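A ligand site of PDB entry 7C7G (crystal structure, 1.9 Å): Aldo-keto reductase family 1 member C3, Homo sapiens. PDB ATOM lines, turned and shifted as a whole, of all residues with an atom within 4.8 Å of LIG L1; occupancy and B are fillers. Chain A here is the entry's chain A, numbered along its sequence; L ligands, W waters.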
ATOM      1  N   TYR A  26       7.923 -23.125  36.865  1.00  0.00           N
ATOM      2  CA  TYR A  26       9.294 -22.828  37.239  1.00  0.00           C
ATOM      3  C   TYR A  26       9.341 -21.904  38.444  1.00  0.00           C
ATOM      4  O   TYR A  26       8.615 -20.904  38.484  1.00  0.00           O
ATOM      5  CB  TYR A  26      10.076 -22.154  36.115  1.00  0.00           C
ATOM      6  CG  TYR A  26      11.497 -21.918  36.609  1.00  0.00           C
ATOM      7  CD1 TYR A  26      12.372 -22.992  36.760  1.00  0.00           C
ATOM      8  CD2 TYR A  26      11.946 -20.658  36.970  1.00  0.00           C
ATOM      9  CE1 TYR A  26      13.664 -22.830  37.230  1.00  0.00           C
ATOM     10  CE2 TYR A  26      13.254 -20.476  37.455  1.00  0.00           C
ATOM     11  CZ  TYR A  26      14.105 -21.586  37.569  1.00  0.00           C
ATOM     12  OH  TYR A  26      15.400 -21.474  38.029  1.00  0.00           O
ATOM     13  N   LEU A  56      14.493 -29.454  33.476  1.00  0.00           N
ATOM     14  CA  LEU A  56      15.306 -28.362  33.970  1.00  0.00           C
ATOM     15  C   LEU A  56      14.802 -27.753  35.273  1.00  0.00           C
ATOM     16  O   LEU A  56      15.573 -27.422  36.151  1.00  0.00           O
ATOM     17  CB  LEU A  56      15.393 -27.252  32.918  1.00  0.00           C
ATOM     18  CG  LEU A  56      16.244 -26.046  33.321  1.00  0.00           C
ATOM     19  CD1 LEU A  56      17.640 -26.495  33.691  1.00  0.00           C
ATOM     20  CD2 LEU A  56      16.282 -24.972  32.250  1.00  0.00           C
ATOM     21  N   TYR A  57      13.488 -27.656  35.405  1.00  0.00           N
ATOM     22  CA  TYR A  57      12.873 -27.040  36.578  1.00  0.00           C
ATOM     23  C   TYR A  57      13.086 -27.721  37.933  1.00  0.00           C
ATOM     24  O   TYR A  57      12.817 -27.118  38.955  1.00  0.00           O
ATOM     25  CB  TYR A  57      11.383 -26.806  36.342  1.00  0.00           C
ATOM     26  CG  TYR A  57      11.050 -26.063  35.080  1.00  0.00           C
ATOM     27  CD1 TYR A  57      12.009 -25.396  34.355  1.00  0.00           C
ATOM     28  CD2 TYR A  57       9.752 -26.025  34.620  1.00  0.00           C
ATOM     29  CE1 TYR A  57      11.696 -24.722  33.184  1.00  0.00           C
ATOM     30  CE2 TYR A  57       9.421 -25.363  33.474  1.00  0.00           C
ATOM     31  CZ  TYR A  57      10.389 -24.706  32.753  1.00  0.00           C
ATOM     32  OH  TYR A  57      10.036 -24.041  31.613  1.00  0.00           O
ATOM     33  N   TRP A  88      15.721 -31.649  27.889  1.00  0.00           N
ATOM     34  CA  TRP A  88      16.783 -30.689  28.136  1.00  0.00           C
ATOM     35  C   TRP A  88      17.900 -30.858  27.117  1.00  0.00           C
ATOM     36  O   TRP A  88      18.072 -31.910  26.506  1.00  0.00           O
ATOM     37  CB  TRP A  88      17.308 -30.846  29.578  1.00  0.00           C
ATOM     38  CG  TRP A  88      18.455 -29.920  29.919  1.00  0.00           C
ATOM     39  CD1 TRP A  88      19.679 -30.274  30.404  1.00  0.00           C
ATOM     40  CD2 TRP A  88      18.472 -28.489  29.801  1.00  0.00           C
ATOM     41  NE1 TRP A  88      20.458 -29.159  30.579  1.00  0.00           N
ATOM     42  CE2 TRP A  88      19.747 -28.042  30.211  1.00  0.00           C
ATOM     43  CE3 TRP A  88      17.532 -27.538  29.359  1.00  0.00           C
ATOM     44  CZ2 TRP A  88      20.109 -26.704  30.214  1.00  0.00           C
ATOM     45  CZ3 TRP A  88      17.894 -26.200  29.362  1.00  0.00           C
ATOM     46  CH2 TRP A  88      19.173 -25.791  29.790  1.00  0.00           C
ATOM     47  N   SER A  89      18.697 -29.787  26.948  1.00  0.00           N
ATOM     48  CA  SER A  89      19.641 -29.691  25.824  1.00  0.00           C
ATOM     49  C   SER A  89      20.840 -30.628  25.942  1.00  0.00           C
ATOM     50  O   SER A  89      21.539 -30.859  24.928  1.00  0.00           O
ATOM     51  CB  SER A  89      20.140 -28.252  25.680  1.00  0.00           C
ATOM     52  OG  SER A  89      19.068 -27.367  25.413  1.00  0.00           O
ATOM     53  N   HIS A 119      13.423 -28.505  24.504  1.00  0.00           N
ATOM     54  CA  HIS A 119      13.400 -27.307  25.354  1.00  0.00           C
ATOM     55  C   HIS A 119      14.080 -26.130  24.660  1.00  0.00           C
ATOM     56  O   HIS A 119      13.616 -24.988  24.770  1.00  0.00           O
ATOM     57  CB  HIS A 119      14.067 -27.574  26.703  1.00  0.00           C
ATOM     58  CG  HIS A 119      13.610 -26.658  27.794  1.00  0.00           C
ATOM     59  ND1 HIS A 119      13.660 -26.992  29.127  1.00  0.00           N
ATOM     60  CD2 HIS A 119      13.068 -25.413  27.736  1.00  0.00           C
ATOM     61  CE1 HIS A 119      13.183 -26.005  29.858  1.00  0.00           C
ATOM     62  NE2 HIS A 119      12.820 -25.030  29.044  1.00  0.00           N
ATOM     63  N   SER A 120      15.167 -26.393  23.936  1.00  0.00           N
ATOM     64  CA  SER A 120      15.897 -25.348  23.247  1.00  0.00           C
ATOM     65  C   SER A 120      16.635 -25.942  22.056  1.00  0.00           C
ATOM     66  O   SER A 120      16.943 -27.136  22.064  1.00  0.00           O
ATOM     67  CB  SER A 120      16.898 -24.659  24.175  1.00  0.00           C
ATOM     68  OG  SER A 120      17.815 -23.858  23.441  1.00  0.00           O
ATOM     69  N   MET A 122      19.695 -25.137  21.208  1.00  0.00           N
ATOM     70  CA  MET A 122      21.127 -25.105  21.480  1.00  0.00           C
ATOM     71  C   MET A 122      21.540 -26.349  22.264  1.00  0.00           C
ATOM     72  O   MET A 122      21.375 -26.425  23.486  1.00  0.00           O
ATOM     73  CB  MET A 122      21.481 -23.827  22.245  1.00  0.00           C
ATOM     74  CG  MET A 122      20.848 -22.576  21.653  1.00  0.00           C
ATOM     75  SD  MET A 122      21.691 -21.092  22.221  1.00  0.00           S
ATOM     76  CE  MET A 122      20.685 -20.621  23.637  1.00  0.00           C
ATOM     77  N   LEU A 124      23.770 -29.215  24.115  1.00  0.00           N
ATOM     78  CA  LEU A 124      24.842 -29.177  25.106  1.00  0.00           C
ATOM     79  C   LEU A 124      25.527 -30.532  25.200  1.00  0.00           C
ATOM     80  O   LEU A 124      25.036 -31.556  24.715  1.00  0.00           O
ATOM     81  CB  LEU A 124      24.315 -28.762  26.489  1.00  0.00           C
ATOM     82  CG  LEU A 124      23.782 -27.334  26.503  1.00  0.00           C
ATOM     83  CD1 LEU A 124      23.411 -26.866  27.897  1.00  0.00           C
ATOM     84  CD2 LEU A 124      24.813 -26.419  25.888  1.00  0.00           C
ATOM     85  N   PHE A 141      29.367 -26.871  24.405  1.00  0.00           N
ATOM     86  CA  PHE A 141      28.306 -27.132  23.448  1.00  0.00           C
ATOM     87  C   PHE A 141      28.440 -28.531  22.855  1.00  0.00           C
ATOM     88  O   PHE A 141      29.475 -29.194  22.979  1.00  0.00           O
ATOM     89  CB  PHE A 141      28.299 -26.087  22.333  1.00  0.00           C
ATOM     90  CG  PHE A 141      28.108 -24.657  22.796  1.00  0.00           C
ATOM     91  CD1 PHE A 141      27.793 -24.367  24.118  1.00  0.00           C
ATOM     92  CD2 PHE A 141      28.219 -23.613  21.895  1.00  0.00           C
ATOM     93  CE1 PHE A 141      27.617 -23.056  24.525  1.00  0.00           C
ATOM     94  CE2 PHE A 141      28.041 -22.292  22.306  1.00  0.00           C
ATOM     95  CZ  PHE A 141      27.744 -22.019  23.624  1.00  0.00           C
ATOM     96  N   ASN A 169      11.613 -22.291  21.790  1.00  0.00           N
ATOM     97  CA  ASN A 169      12.719 -21.356  21.558  1.00  0.00           C
ATOM     98  C   ASN A 169      13.332 -21.505  20.172  1.00  0.00           C
ATOM     99  O   ASN A 169      14.517 -21.214  19.985  1.00  0.00           O
ATOM    100  CB  ASN A 169      13.814 -21.488  22.620  1.00  0.00           C
ATOM    101  CG  ASN A 169      13.350 -21.027  23.972  1.00  0.00           C
ATOM    102  OD1 ASN A 169      12.790 -19.933  24.100  1.00  0.00           O
ATOM    103  ND2 ASN A 169      13.575 -21.855  24.998  1.00  0.00           N
ATOM    104  N   TRP A 229      19.670 -14.108  35.240  1.00  0.00           N
ATOM    105  CA  TRP A 229      19.393 -14.022  33.820  1.00  0.00           C
ATOM    106  C   TRP A 229      18.840 -12.699  33.291  1.00  0.00           C
ATOM    107  O   TRP A 229      18.990 -12.405  32.115  1.00  0.00           O
ATOM    108  CB  TRP A 229      18.422 -15.128  33.425  1.00  0.00           C
ATOM    109  CG  TRP A 229      18.785 -16.474  33.897  1.00  0.00           C
ATOM    110  CD1 TRP A 229      19.973 -17.111  33.721  1.00  0.00           C
ATOM    111  CD2 TRP A 229      17.943 -17.390  34.606  1.00  0.00           C
ATOM    112  NE1 TRP A 229      19.925 -18.356  34.294  1.00  0.00           N
ATOM    113  CE2 TRP A 229      18.696 -18.550  34.843  1.00  0.00           C
ATOM    114  CE3 TRP A 229      16.632 -17.330  35.079  1.00  0.00           C
ATOM    115  CZ2 TRP A 229      18.178 -19.643  35.521  1.00  0.00           C
ATOM    116  CZ3 TRP A 229      16.122 -18.418  35.751  1.00  0.00           C
ATOM    117  CH2 TRP A 229      16.889 -19.558  35.967  1.00  0.00           C
ATOM    118  N   PHE A 308      15.162 -12.588  28.784  1.00  0.00           N
ATOM    119  CA  PHE A 308      16.215 -13.555  29.027  1.00  0.00           C
ATOM    120  C   PHE A 308      17.467 -13.123  28.263  1.00  0.00           C
ATOM    121  O   PHE A 308      17.480 -13.119  27.024  1.00  0.00           O
ATOM    122  CB  PHE A 308      15.771 -14.955  28.603  1.00  0.00           C
ATOM    123  CG  PHE A 308      14.933 -15.659  29.651  1.00  0.00           C
ATOM    124  CD1 PHE A 308      13.581 -15.375  29.777  1.00  0.00           C
ATOM    125  CD2 PHE A 308      15.501 -16.617  30.483  1.00  0.00           C
ATOM    126  CE1 PHE A 308      12.801 -16.022  30.722  1.00  0.00           C
ATOM    127  CE2 PHE A 308      14.729 -17.274  31.433  1.00  0.00           C
ATOM    128  CZ  PHE A 308      13.376 -16.976  31.549  1.00  0.00           C
ATOM    129  N   PHE A 313      25.652 -17.037  24.898  1.00  0.00           N
ATOM    130  CA  PHE A 313      25.698 -18.264  24.116  1.00  0.00           C
ATOM    131  C   PHE A 313      25.621 -17.957  22.620  1.00  0.00           C
ATOM    132  O   PHE A 313      25.302 -18.851  21.822  1.00  0.00           O
ATOM    133  CB  PHE A 313      24.565 -19.190  24.566  1.00  0.00           C
ATOM    134  CG  PHE A 313      24.483 -19.327  26.061  1.00  0.00           C
ATOM    135  CD1 PHE A 313      25.430 -20.077  26.748  1.00  0.00           C
ATOM    136  CD2 PHE A 313      23.485 -18.688  26.784  1.00  0.00           C
ATOM    137  CE1 PHE A 313      25.375 -20.210  28.119  1.00  0.00           C
ATOM    138  CE2 PHE A 313      23.418 -18.806  28.166  1.00  0.00           C
ATOM    139  CZ  PHE A 313      24.363 -19.574  28.839  1.00  0.00           C
ATOM    140  N   HIS A 316      26.676 -20.229  19.685  1.00  0.00           N
ATOM    141  CA  HIS A 316      26.069 -21.512  19.384  1.00  0.00           C
ATOM    142  C   HIS A 316      25.447 -21.522  17.994  1.00  0.00           C
ATOM    143  O   HIS A 316      24.619 -20.665  17.681  1.00  0.00           O
ATOM    144  CB  HIS A 316      25.007 -21.864  20.421  1.00  0.00           C
ATOM    145  CG  HIS A 316      24.670 -23.319  20.432  1.00  0.00           C
ATOM    146  ND1 HIS A 316      24.001 -23.929  19.390  1.00  0.00           N
ATOM    147  CD2 HIS A 316      24.931 -24.294  21.341  1.00  0.00           C
ATOM    148  CE1 HIS A 316      23.855 -25.213  19.661  1.00  0.00           C
ATOM    149  NE2 HIS A 316      24.415 -25.459  20.841  1.00  0.00           N
HETATM  150  C1  LIG L   1      15.155 -20.736  32.618  1.00  0.00           C
HETATM  151  C2  LIG L   1      13.896 -20.787  33.199  1.00  0.00           C
HETATM  152  C3  LIG L   1      12.880 -21.509  32.589  1.00  0.00           C
HETATM  153  C4  LIG L   1      13.135 -22.168  31.403  1.00  0.00           C
HETATM  154  C5  LIG L   1      21.087 -24.050  25.907  1.00  0.00           C
HETATM  155  C6  LIG L   1      22.096 -23.081  25.926  1.00  0.00           C
HETATM  156  C7  LIG L   1      21.892 -21.862  26.562  1.00  0.00           C
HETATM  157  C8  LIG L   1      20.679 -21.599  27.169  1.00  0.00           C
HETATM  158  C9  LIG L   1      19.877 -23.779  26.525  1.00  0.00           C
HETATM  159  C10 LIG L   1      19.678 -22.552  27.171  1.00  0.00           C
HETATM  160  C11 LIG L   1      18.325 -21.953  29.042  1.00  0.00           C
HETATM  161  C12 LIG L   1      16.953 -22.005  29.650  1.00  0.00           C
HETATM  162  C13 LIG L   1      16.688 -21.344  30.859  1.00  0.00           C
HETATM  163  C14 LIG L   1      15.411 -21.405  31.428  1.00  0.00           C
HETATM  164  C15 LIG L   1      14.395 -22.127  30.818  1.00  0.00           C
HETATM  165  C16 LIG L   1      15.845 -22.761  29.019  1.00  0.00           C
HETATM  166  C17 LIG L   1      23.414 -23.345  25.262  1.00  0.00           C
HETATM  167  N1  LIG L   1      18.483 -22.300  27.761  1.00  0.00           N
HETATM  168  N2  LIG L   1      16.055 -23.437  27.852  1.00  0.00           N
HETATM  169  O1  LIG L   1      14.615 -22.794  29.632  1.00  0.00           O
HETATM  170  O2  LIG L   1      12.148 -22.894  30.794  1.00  0.00           O
HETATM  171  O3  LIG L   1      19.257 -21.606  29.753  1.00  0.00           O
HETATM  172  P1  LG2 L   2       5.614 -15.265  34.081  1.00  0.00           P
HETATM  173  O1  LG2 L   2       6.111 -14.123  33.207  1.00  0.00           O
HETATM  174  O2  LG2 L   2       4.383 -16.058  33.673  1.00  0.00           O
HETATM  175  O3  LG2 L   2       5.277 -14.613  35.528  1.00  0.00           O
HETATM  176  C1  LG2 L   2       6.133 -13.597  36.053  1.00  0.00           C
HETATM  177  C2  LG2 L   2       5.778 -13.168  37.480  1.00  0.00           C
HETATM  178  O4  LG2 L   2       4.542 -12.451  37.513  1.00  0.00           O
HETATM  179  C3  LG2 L   2       5.564 -14.338  38.431  1.00  0.00           C
HETATM  180  O5  LG2 L   2       6.725 -14.638  39.170  1.00  0.00           O
HETATM  181  C4  LG2 L   2       4.445 -13.918  39.374  1.00  0.00           C
HETATM  182  O6  LG2 L   2       4.933 -13.744  40.703  1.00  0.00           O
HETATM  183  C5  LG2 L   2       3.933 -12.627  38.808  1.00  0.00           C
HETATM  184  N1  LG2 L   2       2.467 -12.752  38.665  1.00  0.00           N
HETATM  185  C6  LG2 L   2       1.777 -13.877  38.351  1.00  0.00           C
HETATM  186  N2  LG2 L   2       0.437 -13.626  38.294  1.00  0.00           N
HETATM  187  C7  LG2 L   2       0.263 -12.312  38.597  1.00  0.00           C
HETATM  188  C8  LG2 L   2      -0.886 -11.394  38.733  1.00  0.00           C
HETATM  189  N3  LG2 L   2      -2.135 -11.837  38.522  1.00  0.00           N
HETATM  190  N4  LG2 L   2      -0.625 -10.099  39.057  1.00  0.00           N
HETATM  191  C9  LG2 L   2       0.622  -9.647  39.271  1.00  0.00           C
HETATM  192  N5  LG2 L   2       1.712 -10.430  39.177  1.00  0.00           N
HETATM  193  C10 LG2 L   2       1.601 -11.744  38.846  1.00  0.00           C
HETATM  194  O7  LG2 L   2       6.847 -16.144  34.569  1.00  0.00           O
HETATM  195  P2  LG2 L   2       7.843 -17.101  33.734  1.00  0.00           P
HETATM  196  O8  LG2 L   2       8.329 -18.043  34.790  1.00  0.00           O
HETATM  197  O9  LG2 L   2       8.877 -16.264  33.001  1.00  0.00           O
HETATM  198  O10 LG2 L   2       6.923 -17.783  32.613  1.00  0.00           O
HETATM  199  C11 LG2 L   2       5.921 -18.701  32.996  1.00  0.00           C
HETATM  200  C12 LG2 L   2       6.308 -20.134  32.672  1.00  0.00           C
HETATM  201  O11 LG2 L   2       6.812 -20.294  31.347  1.00  0.00           O
HETATM  202  C13 LG2 L   2       7.395 -20.694  33.559  1.00  0.00           C
HETATM  203  O12 LG2 L   2       6.934 -20.939  34.904  1.00  0.00           O
HETATM  204  C14 LG2 L   2       7.861 -21.900  32.766  1.00  0.00           C
HETATM  205  O13 LG2 L   2       6.935 -22.984  32.985  1.00  0.00           O
HETATM  206  C15 LG2 L   2       7.715 -21.412  31.327  1.00  0.00           C
HETATM  207  N6  LG2 L   2       8.980 -20.947  30.764  1.00  0.00           N
HETATM  208  C16 LG2 L   2       9.459 -21.553  29.663  1.00  0.00           C
HETATM  209  C17 LG2 L   2      10.664 -21.150  29.088  1.00  0.00           C
HETATM  210  C18 LG2 L   2      11.207 -21.853  27.869  1.00  0.00           C
HETATM  211  O14 LG2 L   2      12.391 -21.714  27.619  1.00  0.00           O
HETATM  212  N7  LG2 L   2      10.399 -22.599  27.112  1.00  0.00           N
HETATM  213  C19 LG2 L   2      11.377 -20.109  29.668  1.00  0.00           C
HETATM  214  C20 LG2 L   2      10.862 -19.475  30.790  1.00  0.00           C
HETATM  215  C21 LG2 L   2       9.649 -19.916  31.314  1.00  0.00           C
HETATM  216  P3  LG2 L   2       4.233 -14.534  41.937  1.00  0.00           P
HETATM  217  O15 LG2 L   2       4.797 -15.928  41.877  1.00  0.00           O
HETATM  218  O16 LG2 L   2       4.693 -13.732  43.138  1.00  0.00           O
HETATM  219  O17 LG2 L   2       2.747 -14.398  41.643  1.00  0.00           O
HETATM  220  O   HOH W   1      22.186 -23.214  30.158  1.00  0.00           O
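O2 of LIG L1 is in hydrogen-bond range of OH of Tyr 57 (2.5 Å). A ring nitrogen (NE2) of His 119 lies within hydrogen-bond range of an oxygen (O2) of LIG L1, 2.8 Å away. The side-chain amide nitrogen of Asn 169 lies within hydrogen-bond range of an oxygen (O14) of LG2 L2 (2.9 Å). The backbone NH (N) of Tyr 26 lies within hydrogen-bond range of an oxygen (O12) of LG2 L2 (3.1 Å).
An oxygen (O2) of LIG L1 lies close to an oxygen (O14) of LG2 L2.
ND2 of Asn 169 is in hydrogen-bond range of O of His 119, at 3.1 Å. The backbone NH of Met 122 is in hydrogen-bond range of the side-chain hydroxyl of Ser 120. The side-chain hydroxyl of Ser 89 sits close to the backbone carbonyl oxygen of Met 122 (3.2 Å). N of Leu 124 lies within hydrogen-bond range of O of Ser 89.
Residues that only touch LIG L1: Leu 56, Trp 88, Ser 89, Ser 120, Met 122, Leu 124, Trp 229, Phe 308 and Phe 313. Of the 15 residues printed, 11 come within 4 Å of LIG L1. The nearest printed residue that does not touch LIG L1 is Asn 169 (4.1 Å).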
